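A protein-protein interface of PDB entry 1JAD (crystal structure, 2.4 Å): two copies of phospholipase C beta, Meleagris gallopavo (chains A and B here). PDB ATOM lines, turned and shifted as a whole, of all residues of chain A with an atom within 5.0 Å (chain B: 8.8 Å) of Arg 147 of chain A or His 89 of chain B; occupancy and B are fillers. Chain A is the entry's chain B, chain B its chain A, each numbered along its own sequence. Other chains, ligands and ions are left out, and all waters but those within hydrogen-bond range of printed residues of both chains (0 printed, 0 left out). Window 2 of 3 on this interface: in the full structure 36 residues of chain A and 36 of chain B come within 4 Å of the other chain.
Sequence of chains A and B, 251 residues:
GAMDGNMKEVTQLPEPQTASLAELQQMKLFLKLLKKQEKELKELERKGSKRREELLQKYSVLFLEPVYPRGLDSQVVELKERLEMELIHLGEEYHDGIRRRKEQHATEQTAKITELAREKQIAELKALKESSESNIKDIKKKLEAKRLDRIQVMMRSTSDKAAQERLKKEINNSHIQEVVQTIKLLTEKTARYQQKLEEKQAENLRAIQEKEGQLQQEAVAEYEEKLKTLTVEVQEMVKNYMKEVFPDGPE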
ATOM      1  N   LEU A 143     -39.149  -8.576  16.888  1.00  0.00           N
ATOM      2  CA  LEU A 143     -38.690  -9.512  15.857  1.00  0.00           C
ATOM      3  C   LEU A 143     -38.104 -10.802  16.413  1.00  0.00           C
ATOM      4  O   LEU A 143     -38.314 -11.887  15.858  1.00  0.00           O
ATOM      5  CB  LEU A 143     -37.625  -8.847  14.988  1.00  0.00           C
ATOM      6  CG  LEU A 143     -38.019  -7.611  14.194  1.00  0.00           C
ATOM      7  CD1 LEU A 143     -36.788  -7.042  13.516  1.00  0.00           C
ATOM      8  CD2 LEU A 143     -39.093  -7.976  13.186  1.00  0.00           C
ATOM      9  N   GLU A 144     -37.348 -10.671  17.494  1.00  0.00           N
ATOM     10  CA  GLU A 144     -36.715 -11.814  18.111  1.00  0.00           C
ATOM     11  C   GLU A 144     -37.784 -12.512  18.935  1.00  0.00           C
ATOM     12  O   GLU A 144     -37.855 -13.742  18.960  1.00  0.00           O
ATOM     13  CB  GLU A 144     -35.534 -11.338  18.967  1.00  0.00           C
ATOM     14  CG  GLU A 144     -34.463 -12.398  19.266  1.00  0.00           C
ATOM     15  CD  GLU A 144     -34.778 -13.240  20.479  1.00  0.00           C
ATOM     16  OE1 GLU A 144     -33.987 -14.157  20.793  1.00  0.00           O
ATOM     17  OE2 GLU A 144     -35.812 -12.974  21.126  1.00  0.00           O
ATOM     18  N   ALA A 145     -38.635 -11.724  19.588  1.00  0.00           N
ATOM     19  CA  ALA A 145     -39.715 -12.289  20.390  1.00  0.00           C
ATOM     20  C   ALA A 145     -40.529 -13.194  19.475  1.00  0.00           C
ATOM     21  O   ALA A 145     -40.985 -14.260  19.890  1.00  0.00           O
ATOM     22  CB  ALA A 145     -40.590 -11.184  20.962  1.00  0.00           C
ATOM     23  N   LYS A 146     -40.711 -12.762  18.231  1.00  0.00           N
ATOM     24  CA  LYS A 146     -41.440 -13.559  17.255  1.00  0.00           C
ATOM     25  C   LYS A 146     -40.624 -14.802  16.942  1.00  0.00           C
ATOM     26  O   LYS A 146     -41.177 -15.874  16.698  1.00  0.00           O
ATOM     27  CB  LYS A 146     -41.681 -12.776  15.960  1.00  0.00           C
ATOM     28  CG  LYS A 146     -43.000 -12.017  15.890  1.00  0.00           C
ATOM     29  CD  LYS A 146     -44.194 -12.976  15.914  1.00  0.00           C
ATOM     30  CE  LYS A 146     -45.517 -12.241  15.726  1.00  0.00           C
ATOM     31  NZ  LYS A 146     -45.724 -11.177  16.745  1.00  0.00           N
ATOM     32  N   ARG A 147     -39.304 -14.659  16.946  1.00  0.00           N
ATOM     33  CA  ARG A 147     -38.446 -15.792  16.654  1.00  0.00           C
ATOM     34  C   ARG A 147     -38.800 -16.934  17.615  1.00  0.00           C
ATOM     35  O   ARG A 147     -39.237 -17.995  17.170  1.00  0.00           O
ATOM     36  CB  ARG A 147     -36.964 -15.397  16.782  1.00  0.00           C
ATOM     37  CG  ARG A 147     -35.990 -16.398  16.158  1.00  0.00           C
ATOM     38  CD  ARG A 147     -34.543 -15.931  16.256  1.00  0.00           C
ATOM     39  NE  ARG A 147     -34.060 -15.891  17.634  1.00  0.00           N
ATOM     40  CZ  ARG A 147     -33.914 -16.964  18.409  1.00  0.00           C
ATOM     41  NH1 ARG A 147     -34.213 -18.166  17.940  1.00  0.00           N
ATOM     42  NH2 ARG A 147     -33.475 -16.835  19.656  1.00  0.00           N
ATOM     43  N   LEU A 148     -38.646 -16.717  18.922  1.00  0.00           N
ATOM     44  CA  LEU A 148     -38.959 -17.758  19.903  1.00  0.00           C
ATOM     45  C   LEU A 148     -40.331 -18.372  19.673  1.00  0.00           C
ATOM     46  O   LEU A 148     -40.515 -19.575  19.846  1.00  0.00           O
ATOM     47  CB  LEU A 148     -38.949 -17.220  21.339  1.00  0.00           C
ATOM     48  CG  LEU A 148     -37.720 -16.633  22.031  1.00  0.00           C
ATOM     49  CD1 LEU A 148     -36.569 -17.626  21.997  1.00  0.00           C
ATOM     50  CD2 LEU A 148     -37.338 -15.341  21.355  1.00  0.00           C
ATOM     51  N   ASP A 149     -41.291 -17.538  19.292  1.00  0.00           N
ATOM     52  CA  ASP A 149     -42.658 -17.994  19.085  1.00  0.00           C
ATOM     53  C   ASP A 149     -42.873 -18.828  17.824  1.00  0.00           C
ATOM     54  O   ASP A 149     -43.637 -19.792  17.847  1.00  0.00           O
ATOM     55  CB  ASP A 149     -43.607 -16.790  19.111  1.00  0.00           C
ATOM     56  CG  ASP A 149     -45.065 -17.196  19.110  1.00  0.00           C
ATOM     57  OD1 ASP A 149     -45.559 -17.629  18.049  1.00  0.00           O
ATOM     58  OD2 ASP A 149     -45.710 -17.095  20.179  1.00  0.00           O
ATOM     59  N   ARG A 150     -42.208 -18.477  16.729  1.00  0.00           N
ATOM     60  CA  ARG A 150     -42.358 -19.248  15.496  1.00  0.00           C
ATOM     61  C   ARG A 150     -41.666 -20.599  15.694  1.00  0.00           C
ATOM     62  O   ARG A 150     -41.856 -21.532  14.911  1.00  0.00           O
ATOM     63  CB  ARG A 150     -41.729 -18.502  14.314  1.00  0.00           C
ATOM     64  CG  ARG A 150     -42.280 -17.107  14.122  1.00  0.00           C
ATOM     65  CD  ARG A 150     -41.577 -16.359  13.004  1.00  0.00           C
ATOM     66  NE  ARG A 150     -41.941 -14.944  13.013  1.00  0.00           N
ATOM     67  CZ  ARG A 150     -41.467 -14.041  12.162  1.00  0.00           C
ATOM     68  NH1 ARG A 150     -40.603 -14.402  11.222  1.00  0.00           N
ATOM     69  NH2 ARG A 150     -41.849 -12.771  12.260  1.00  0.00           N
ATOM     70  N   ILE A 151     -40.859 -20.685  16.751  1.00  0.00           N
ATOM     71  CA  ILE A 151     -40.140 -21.908  17.094  1.00  0.00           C
ATOM     72  C   ILE A 151     -40.958 -22.721  18.095  1.00  0.00           C
ATOM     73  O   ILE A 151     -41.278 -23.879  17.837  1.00  0.00           O
ATOM     74  CB  ILE A 151     -38.763 -21.605  17.729  1.00  0.00           C
ATOM     75  CG1 ILE A 151     -37.890 -20.822  16.749  1.00  0.00           C
ATOM     76  CG2 ILE A 151     -38.077 -22.907  18.123  1.00  0.00           C
ATOM     77  CD1 ILE A 151     -37.592 -21.559  15.463  1.00  0.00           C
ATOM     78  N   ILE A 171     -35.723 -20.576  10.277  1.00  0.00           N
ATOM     79  CA  ILE A 171     -36.418 -19.537  11.032  1.00  0.00           C
ATOM     80  C   ILE A 171     -35.430 -18.523  11.587  1.00  0.00           C
ATOM     81  O   ILE A 171     -35.717 -17.328  11.620  1.00  0.00           O
ATOM     82  CB  ILE A 171     -37.252 -20.128  12.195  1.00  0.00           C
ATOM     83  CG1 ILE A 171     -38.399 -20.971  11.625  1.00  0.00           C
ATOM     84  CG2 ILE A 171     -37.799 -19.007  13.078  1.00  0.00           C
ATOM     85  CD1 ILE A 171     -39.291 -21.604  12.666  1.00  0.00           C
ATOM     86  N   ASN A 172     -34.271 -18.993  12.036  1.00  0.00           N
ATOM     87  CA  ASN A 172     -33.262 -18.080  12.546  1.00  0.00           C
ATOM     88  C   ASN A 172     -32.649 -17.386  11.335  1.00  0.00           C
ATOM     89  O   ASN A 172     -31.748 -16.555  11.454  1.00  0.00           O
ATOM     90  CB  ASN A 172     -32.197 -18.832  13.345  1.00  0.00           C
ATOM     91  CG  ASN A 172     -32.729 -19.365  14.672  1.00  0.00           C
ATOM     92  OD1 ASN A 172     -33.301 -18.617  15.468  1.00  0.00           O
ATOM     93  ND2 ASN A 172     -32.526 -20.655  14.922  1.00  0.00           N
ATOM     94  N   HIS A 175     -35.337 -14.149  10.828  1.00  0.00           N
ATOM     95  CA  HIS A 175     -34.929 -13.151  11.807  1.00  0.00           C
ATOM     96  C   HIS A 175     -33.719 -12.364  11.315  1.00  0.00           C
ATOM     97  O   HIS A 175     -33.812 -11.172  11.024  1.00  0.00           O
ATOM     98  CB  HIS A 175     -34.586 -13.835  13.133  1.00  0.00           C
ATOM     99  CG  HIS A 175     -34.171 -12.887  14.216  1.00  0.00           C
ATOM    100  ND1 HIS A 175     -35.028 -11.955  14.758  1.00  0.00           N
ATOM    101  CD2 HIS A 175     -32.986 -12.723  14.850  1.00  0.00           C
ATOM    102  CE1 HIS A 175     -34.390 -11.255  15.680  1.00  0.00           C
ATOM    103  NE2 HIS A 175     -33.149 -11.701  15.754  1.00  0.00           N
ATOM    104  N   ARG B  51     -15.239 -10.590  26.007  1.00  0.00           N
ATOM    105  CA  ARG B  51     -16.564 -11.132  26.238  1.00  0.00           C
ATOM    106  C   ARG B  51     -16.801 -12.436  25.482  1.00  0.00           C
ATOM    107  O   ARG B  51     -17.476 -13.329  25.994  1.00  0.00           O
ATOM    108  CB  ARG B  51     -17.634 -10.097  25.876  1.00  0.00           C
ATOM    109  CG  ARG B  51     -19.053 -10.636  25.919  1.00  0.00           C
ATOM    110  CD  ARG B  51     -19.327 -11.378  27.217  1.00  0.00           C
ATOM    111  NE  ARG B  51     -20.694 -11.890  27.295  1.00  0.00           N
ATOM    112  CZ  ARG B  51     -21.773 -11.124  27.412  1.00  0.00           C
ATOM    113  NH1 ARG B  51     -21.648  -9.803  27.469  1.00  0.00           N
ATOM    114  NH2 ARG B  51     -22.979 -11.677  27.480  1.00  0.00           N
ATOM    115  N   LEU B  55     -17.062 -16.135  27.146  1.00  0.00           N
ATOM    116  CA  LEU B  55     -18.258 -16.930  26.883  1.00  0.00           C
ATOM    117  C   LEU B  55     -17.877 -18.376  26.566  1.00  0.00           C
ATOM    118  O   LEU B  55     -18.630 -19.305  26.869  1.00  0.00           O
ATOM    119  CB  LEU B  55     -19.051 -16.335  25.709  1.00  0.00           C
ATOM    120  CG  LEU B  55     -20.351 -17.032  25.287  1.00  0.00           C
ATOM    121  CD1 LEU B  55     -21.321 -17.089  26.461  1.00  0.00           C
ATOM    122  CD2 LEU B  55     -20.981 -16.281  24.126  1.00  0.00           C
ATOM    123  N   ARG B  82     -26.940 -24.151  22.212  1.00  0.00           N
ATOM    124  CA  ARG B  82     -27.109 -23.070  23.175  1.00  0.00           C
ATOM    125  C   ARG B  82     -25.929 -22.108  23.101  1.00  0.00           C
ATOM    126  O   ARG B  82     -26.086 -20.901  23.283  1.00  0.00           O
ATOM    127  CB  ARG B  82     -27.219 -23.659  24.575  1.00  0.00           C
ATOM    128  CG  ARG B  82     -27.565 -22.671  25.668  1.00  0.00           C
ATOM    129  CD  ARG B  82     -27.758 -23.435  26.964  1.00  0.00           C
ATOM    130  NE  ARG B  82     -28.699 -24.535  26.766  1.00  0.00           N
ATOM    131  CZ  ARG B  82     -28.991 -25.453  27.682  1.00  0.00           C
ATOM    132  NH1 ARG B  82     -28.414 -25.413  28.879  1.00  0.00           N
ATOM    133  NH2 ARG B  82     -29.854 -26.422  27.394  1.00  0.00           N
ATOM    134  N   LEU B  83     -24.749 -22.665  22.841  1.00  0.00           N
ATOM    135  CA  LEU B  83     -23.516 -21.895  22.716  1.00  0.00           C
ATOM    136  C   LEU B  83     -23.612 -21.021  21.475  1.00  0.00           C
ATOM    137  O   LEU B  83     -23.334 -19.826  21.511  1.00  0.00           O
ATOM    138  CB  LEU B  83     -22.327 -22.840  22.572  1.00  0.00           C
ATOM    139  CG  LEU B  83     -20.967 -22.202  22.298  1.00  0.00           C
ATOM    140  CD1 LEU B  83     -20.582 -21.273  23.437  1.00  0.00           C
ATOM    141  CD2 LEU B  83     -19.926 -23.298  22.132  1.00  0.00           C
ATOM    142  N   GLU B  84     -24.018 -21.647  20.376  1.00  0.00           N
ATOM    143  CA  GLU B  84     -24.172 -20.970  19.102  1.00  0.00           C
ATOM    144  C   GLU B  84     -25.078 -19.753  19.190  1.00  0.00           C
ATOM    145  O   GLU B  84     -24.774 -18.711  18.610  1.00  0.00           O
ATOM    146  CB  GLU B  84     -24.710 -21.948  18.052  1.00  0.00           C
ATOM    147  CG  GLU B  84     -23.703 -23.026  17.671  1.00  0.00           C
ATOM    148  CD  GLU B  84     -24.207 -23.970  16.592  1.00  0.00           C
ATOM    149  OE1 GLU B  84     -24.629 -23.488  15.516  1.00  0.00           O
ATOM    150  OE2 GLU B  84     -24.165 -25.198  16.810  1.00  0.00           O
ATOM    151  N   MET B  85     -26.176 -19.877  19.931  1.00  0.00           N
ATOM    152  CA  MET B  85     -27.118 -18.776  20.058  1.00  0.00           C
ATOM    153  C   MET B  85     -26.613 -17.648  20.960  1.00  0.00           C
ATOM    154  O   MET B  85     -26.959 -16.486  20.746  1.00  0.00           O
ATOM    155  CB  MET B  85     -28.474 -19.292  20.552  1.00  0.00           C
ATOM    156  CG  MET B  85     -29.630 -18.312  20.316  1.00  0.00           C
ATOM    157  SD  MET B  85     -29.843 -17.817  18.538  1.00  0.00           S
ATOM    158  CE  MET B  85     -30.013 -19.472  17.729  1.00  0.00           C
ATOM    159  N   GLU B  86     -25.804 -17.972  21.965  1.00  0.00           N
ATOM    160  CA  GLU B  86     -25.268 -16.928  22.831  1.00  0.00           C
ATOM    161  C   GLU B  86     -24.167 -16.170  22.102  1.00  0.00           C
ATOM    162  O   GLU B  86     -23.885 -15.009  22.412  1.00  0.00           O
ATOM    163  CB  GLU B  86     -24.731 -17.510  24.133  1.00  0.00           C
ATOM    164  CG  GLU B  86     -25.819 -17.861  25.130  1.00  0.00           C
ATOM    165  CD  GLU B  86     -25.257 -18.338  26.457  1.00  0.00           C
ATOM    166  OE1 GLU B  86     -24.403 -17.628  27.037  1.00  0.00           O
ATOM    167  OE2 GLU B  86     -25.678 -19.420  26.924  1.00  0.00           O
ATOM    168  N   LEU B  87     -23.536 -16.833  21.139  1.00  0.00           N
ATOM    169  CA  LEU B  87     -22.511 -16.182  20.346  1.00  0.00           C
ATOM    170  C   LEU B  87     -23.236 -15.307  19.332  1.00  0.00           C
ATOM    171  O   LEU B  87     -22.852 -14.168  19.110  1.00  0.00           O
ATOM    172  CB  LEU B  87     -21.628 -17.208  19.631  1.00  0.00           C
ATOM    173  CG  LEU B  87     -20.635 -17.962  20.527  1.00  0.00           C
ATOM    174  CD1 LEU B  87     -19.916 -19.018  19.692  1.00  0.00           C
ATOM    175  CD2 LEU B  87     -19.636 -16.982  21.150  1.00  0.00           C
ATOM    176  N   ILE B  88     -24.290 -15.841  18.723  1.00  0.00           N
ATOM    177  CA  ILE B  88     -25.064 -15.063  17.766  1.00  0.00           C
ATOM    178  C   ILE B  88     -25.532 -13.778  18.454  1.00  0.00           C
ATOM    179  O   ILE B  88     -25.280 -12.673  17.962  1.00  0.00           O
ATOM    180  CB  ILE B  88     -26.304 -15.831  17.277  1.00  0.00           C
ATOM    181  CG1 ILE B  88     -25.885 -17.015  16.405  1.00  0.00           C
ATOM    182  CG2 ILE B  88     -27.219 -14.892  16.491  1.00  0.00           C
ATOM    183  CD1 ILE B  88     -25.272 -16.612  15.094  1.00  0.00           C
ATOM    184  N   HIS B  89     -26.211 -13.920  19.592  1.00  0.00           N
ATOM    185  CA  HIS B  89     -26.680 -12.752  20.320  1.00  0.00           C
ATOM    186  C   HIS B  89     -25.541 -11.817  20.663  1.00  0.00           C
ATOM    187  O   HIS B  89     -25.680 -10.597  20.557  1.00  0.00           O
ATOM    188  CB  HIS B  89     -27.435 -13.161  21.584  1.00  0.00           C
ATOM    189  CG  HIS B  89     -28.807 -13.696  21.309  1.00  0.00           C
ATOM    190  ND1 HIS B  89     -29.691 -14.040  22.310  1.00  0.00           N
ATOM    191  CD2 HIS B  89     -29.453 -13.930  20.141  1.00  0.00           C
ATOM    192  CE1 HIS B  89     -30.821 -14.462  21.769  1.00  0.00           C
ATOM    193  NE2 HIS B  89     -30.705 -14.405  20.455  1.00  0.00           N
ATOM    194  N   LEU B  90     -24.407 -12.375  21.069  1.00  0.00           N
ATOM    195  CA  LEU B  90     -23.254 -11.536  21.386  1.00  0.00           C
ATOM    196  C   LEU B  90     -22.835 -10.761  20.138  1.00  0.00           C
ATOM    197  O   LEU B  90     -22.431  -9.603  20.219  1.00  0.00           O
ATOM    198  CB  LEU B  90     -22.071 -12.381  21.857  1.00  0.00           C
ATOM    199  CG  LEU B  90     -20.818 -11.533  22.068  1.00  0.00           C
ATOM    200  CD1 LEU B  90     -21.109 -10.486  23.123  1.00  0.00           C
ATOM    201  CD2 LEU B  90     -19.645 -12.404  22.469  1.00  0.00           C
ATOM    202  N   GLY B  91     -22.919 -11.417  18.985  1.00  0.00           N
ATOM    203  CA  GLY B  91     -22.549 -10.763  17.745  1.00  0.00           C
ATOM    204  C   GLY B  91     -23.506  -9.627  17.443  1.00  0.00           C
ATOM    205  O   GLY B  91     -23.088  -8.528  17.062  1.00  0.00           O
ATOM    206  N   GLU B  92     -24.796  -9.892  17.636  1.00  0.00           N
ATOM    207  CA  GLU B  92     -25.836  -8.898  17.379  1.00  0.00           C
ATOM    208  C   GLU B  92     -25.653  -7.614  18.182  1.00  0.00           C
ATOM    209  O   GLU B  92     -25.722  -6.518  17.620  1.00  0.00           O
ATOM    210  CB  GLU B  92     -27.226  -9.490  17.659  1.00  0.00           C
ATOM    211  CG  GLU B  92     -27.645 -10.603  16.681  1.00  0.00           C
ATOM    212  CD  GLU B  92     -29.025 -11.200  16.984  1.00  0.00           C
ATOM    213  OE1 GLU B  92     -29.529 -11.986  16.152  1.00  0.00           O
ATOM    214  OE2 GLU B  92     -29.607 -10.896  18.052  1.00  0.00           O
ATOM    215  N   GLU B  93     -25.404  -7.735  19.485  1.00  0.00           N
ATOM    216  CA  GLU B  93     -25.238  -6.546  20.307  1.00  0.00           C
ATOM    217  C   GLU B  93     -23.887  -5.890  20.029  1.00  0.00           C
ATOM    218  O   GLU B  93     -23.768  -4.666  20.067  1.00  0.00           O
ATOM    219  CB  GLU B  93     -25.358  -6.897  21.800  1.00  0.00           C
ATOM    220  CG  GLU B  93     -25.939  -5.768  22.691  1.00  0.00           C
ATOM    221  CD  GLU B  93     -25.184  -4.433  22.591  1.00  0.00           C
ATOM    222  OE1 GLU B  93     -23.975  -4.391  22.924  1.00  0.00           O
ATOM    223  OE2 GLU B  93     -25.806  -3.422  22.183  1.00  0.00           O
ATOM    224  N   TYR B  94     -22.874  -6.706  19.745  1.00  0.00           N
ATOM    225  CA  TYR B  94     -21.532  -6.200  19.467  1.00  0.00           C
ATOM    226  C   TYR B  94     -21.455  -5.299  18.226  1.00  0.00           C
ATOM    227  O   TYR B  94     -20.951  -4.168  18.284  1.00  0.00           O
ATOM    228  CB  TYR B  94     -20.553  -7.366  19.297  1.00  0.00           C
ATOM    229  CG  TYR B  94     -19.172  -6.944  18.821  1.00  0.00           C
ATOM    230  CD1 TYR B  94     -18.360  -6.117  19.601  1.00  0.00           C
ATOM    231  CD2 TYR B  94     -18.697  -7.335  17.564  1.00  0.00           C
ATOM    232  CE1 TYR B  94     -17.113  -5.683  19.140  1.00  0.00           C
ATOM    233  CE2 TYR B  94     -17.452  -6.907  17.093  1.00  0.00           C
ATOM    234  CZ  TYR B  94     -16.668  -6.077  17.884  1.00  0.00           C
ATOM    235  OH  TYR B  94     -15.460  -5.609  17.399  1.00  0.00           O
ATOM    236  N   HIS B  95     -21.936  -5.803  17.097  1.00  0.00           N
ATOM    237  CA  HIS B  95     -21.893  -5.026  15.874  1.00  0.00           C
ATOM    238  C   HIS B  95     -22.827  -3.831  15.962  1.00  0.00           C
ATOM    239  O   HIS B  95     -22.464  -2.733  15.537  1.00  0.00           O
ATOM    240  CB  HIS B  95     -22.237  -5.922  14.693  1.00  0.00           C
ATOM    241  CG  HIS B  95     -21.250  -7.030  14.485  1.00  0.00           C
ATOM    242  ND1 HIS B  95     -19.935  -6.797  14.143  1.00  0.00           N
ATOM    243  CD2 HIS B  95     -21.375  -8.374  14.605  1.00  0.00           C
ATOM    244  CE1 HIS B  95     -19.293  -7.949  14.062  1.00  0.00           C
ATOM    245  NE2 HIS B  95     -20.144  -8.920  14.339  1.00  0.00           N
ATOM    246  N   ASP B  96     -24.020  -4.036  16.524  1.00  0.00           N
ATOM    247  CA  ASP B  96     -24.974  -2.943  16.687  1.00  0.00           C
ATOM    248  C   ASP B  96     -24.281  -1.837  17.468  1.00  0.00           C
ATOM    249  O   ASP B  96     -24.454  -0.649  17.175  1.00  0.00           O
ATOM    250  CB  ASP B  96     -26.216  -3.411  17.447  1.00  0.00           C
ATOM    251  CG  ASP B  96     -27.146  -2.260  17.824  1.00  0.00           C
ATOM    252  OD1 ASP B  96     -26.717  -1.371  18.597  1.00  0.00           O
ATOM    253  OD2 ASP B  96     -28.309  -2.246  17.361  1.00  0.00           O
ATOM    254  N   LEU B 227     -23.826  -8.804  10.113  1.00  0.00           N
ATOM    255  CA  LEU B 227     -24.969  -9.601  10.547  1.00  0.00           C
ATOM    256  C   LEU B 227     -25.330 -10.742   9.585  1.00  0.00           C
ATOM    257  O   LEU B 227     -25.771 -11.807  10.010  1.00  0.00           O
ATOM    258  CB  LEU B 227     -26.179  -8.681  10.745  1.00  0.00           C
ATOM    259  CG  LEU B 227     -27.315  -9.213  11.616  1.00  0.00           C
ATOM    260  CD1 LEU B 227     -26.781  -9.409  13.027  1.00  0.00           C
ATOM    261  CD2 LEU B 227     -28.482  -8.234  11.639  1.00  0.00           C
ATOM    262  N   LEU B 230     -22.650 -13.340  10.158  1.00  0.00           N
ATOM    263  CA  LEU B 230     -22.613 -13.735  11.566  1.00  0.00           C
ATOM    264  C   LEU B 230     -22.956 -15.196  11.845  1.00  0.00           C
ATOM    265  O   LEU B 230     -22.211 -15.878  12.543  1.00  0.00           O
ATOM    266  CB  LEU B 230     -23.550 -12.839  12.388  1.00  0.00           C
ATOM    267  CG  LEU B 230     -23.731 -13.128  13.884  1.00  0.00           C
ATOM    268  CD1 LEU B 230     -22.406 -12.988  14.626  1.00  0.00           C
ATOM    269  CD2 LEU B 230     -24.763 -12.165  14.447  1.00  0.00           C
ATOM    270  N   THR B 231     -24.078 -15.675  11.309  1.00  0.00           N
ATOM    271  CA  THR B 231     -24.505 -17.059  11.531  1.00  0.00           C
ATOM    272  C   THR B 231     -23.452 -18.119  11.198  1.00  0.00           C
ATOM    273  O   THR B 231     -23.345 -19.124  11.890  1.00  0.00           O
ATOM    274  CB  THR B 231     -25.783 -17.380  10.731  1.00  0.00           C
ATOM    275  OG1 THR B 231     -26.851 -16.534  11.169  1.00  0.00           O
ATOM    276  CG2 THR B 231     -26.180 -18.829  10.929  1.00  0.00           C
ATOM    277  N   VAL B 234     -19.894 -18.078  13.331  1.00  0.00           N
ATOM    278  CA  VAL B 234     -20.020 -18.644  14.665  1.00  0.00           C
ATOM    279  C   VAL B 234     -20.103 -20.161  14.632  1.00  0.00           C
ATOM    280  O   VAL B 234     -19.380 -20.837  15.359  1.00  0.00           O
ATOM    281  CB  VAL B 234     -21.253 -18.079  15.408  1.00  0.00           C
ATOM    282  CG1 VAL B 234     -21.070 -16.595  15.650  1.00  0.00           C
ATOM    283  CG2 VAL B 234     -22.514 -18.334  14.608  1.00  0.00           C
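ND1 of His 175 of chain A is in hydrogen-bond range of O of Leu 143 of chain A, 3.5 Å away.
The side-chain carboxylate (OE1) of Glu 144 of chain A is in salt-bridge range of the guanidinium group (NH2) of Arg 147 of chain A, 3.0 Å away.
The side-chain amide oxygen of Asn 172 of chain A is in hydrogen-bond range of the guanidinium group of Arg 147 of chain A (2.7 Å).
NE2 of His 89 of chain B lies within hydrogen-bond range of OE1 of Glu 144 of chain A, 3.3 Å away.
Arg 147 of chain A touches Met 85 of chain B.
His 89 of chain B touches Arg 147 of chain A.
Met 85 of chain B touches Asn 172 of chain A.
His 175 of chain A touches Glu 92 of chain B (NE2 to OE1, 3.7 Å).
Of the 21 printed residues of chain B, 3 touch a printed residue of chain A.
Hydrophobic or aromatic side chains of chain B that line the printed part of chain A: Met 85 and His 89.
Of the 12 printed residues of chain A, 4 touch a printed residue of chain B.
Hydrophobic or aromatic side chains of chain A that line the printed part of chain B: His 175.
Among the printed residues, 5 pairs touch across the chains.
Among the printed residues, no Asp or Glu carboxylate lies within 4 Å of a Lys or Arg side-chain nitrogen of the other chain.
Of the printed residues of chain A, His 89 of chain B touches Glu 144 (3.3 Å) and Arg 147 (3.8 Å).
Printed residues of chain B within 4 Å of Asn 172 of chain A: Met 85.
Printed residues of chain B within 4 Å of His 175 of chain A: Glu 92 (3.7 Å).
Printed residues of chain A within 4 Å of Met 85 of chain B: Arg 147 (3.9 Å) and Asn 172 (3.9 Å).
Printed residues of chain A within 4 Å of Glu 92 of chain B: His 175.
Printed residues of chain B within 4 Å of Glu 144 of chain A: His 89.
Ala 145 of chain A touches none of the printed residues of chain B.
The nearest residue of chain B that does not touch Arg 147 of chain A is Glu 92 of chain B (6.2 Å).
The nearest printed residue of chain A that does not touch His 89 of chain B is His 175 of chain A (5.9 Å).
The nearest printed residue of chain B that does not touch Glu 144 of chain A is Glu 92 of chain B (5.2 Å).
No position is printed for both chains.
Of the 5 pairs that touch across the chains among the printed residues, none has its exchanged pair printed and touching as well.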
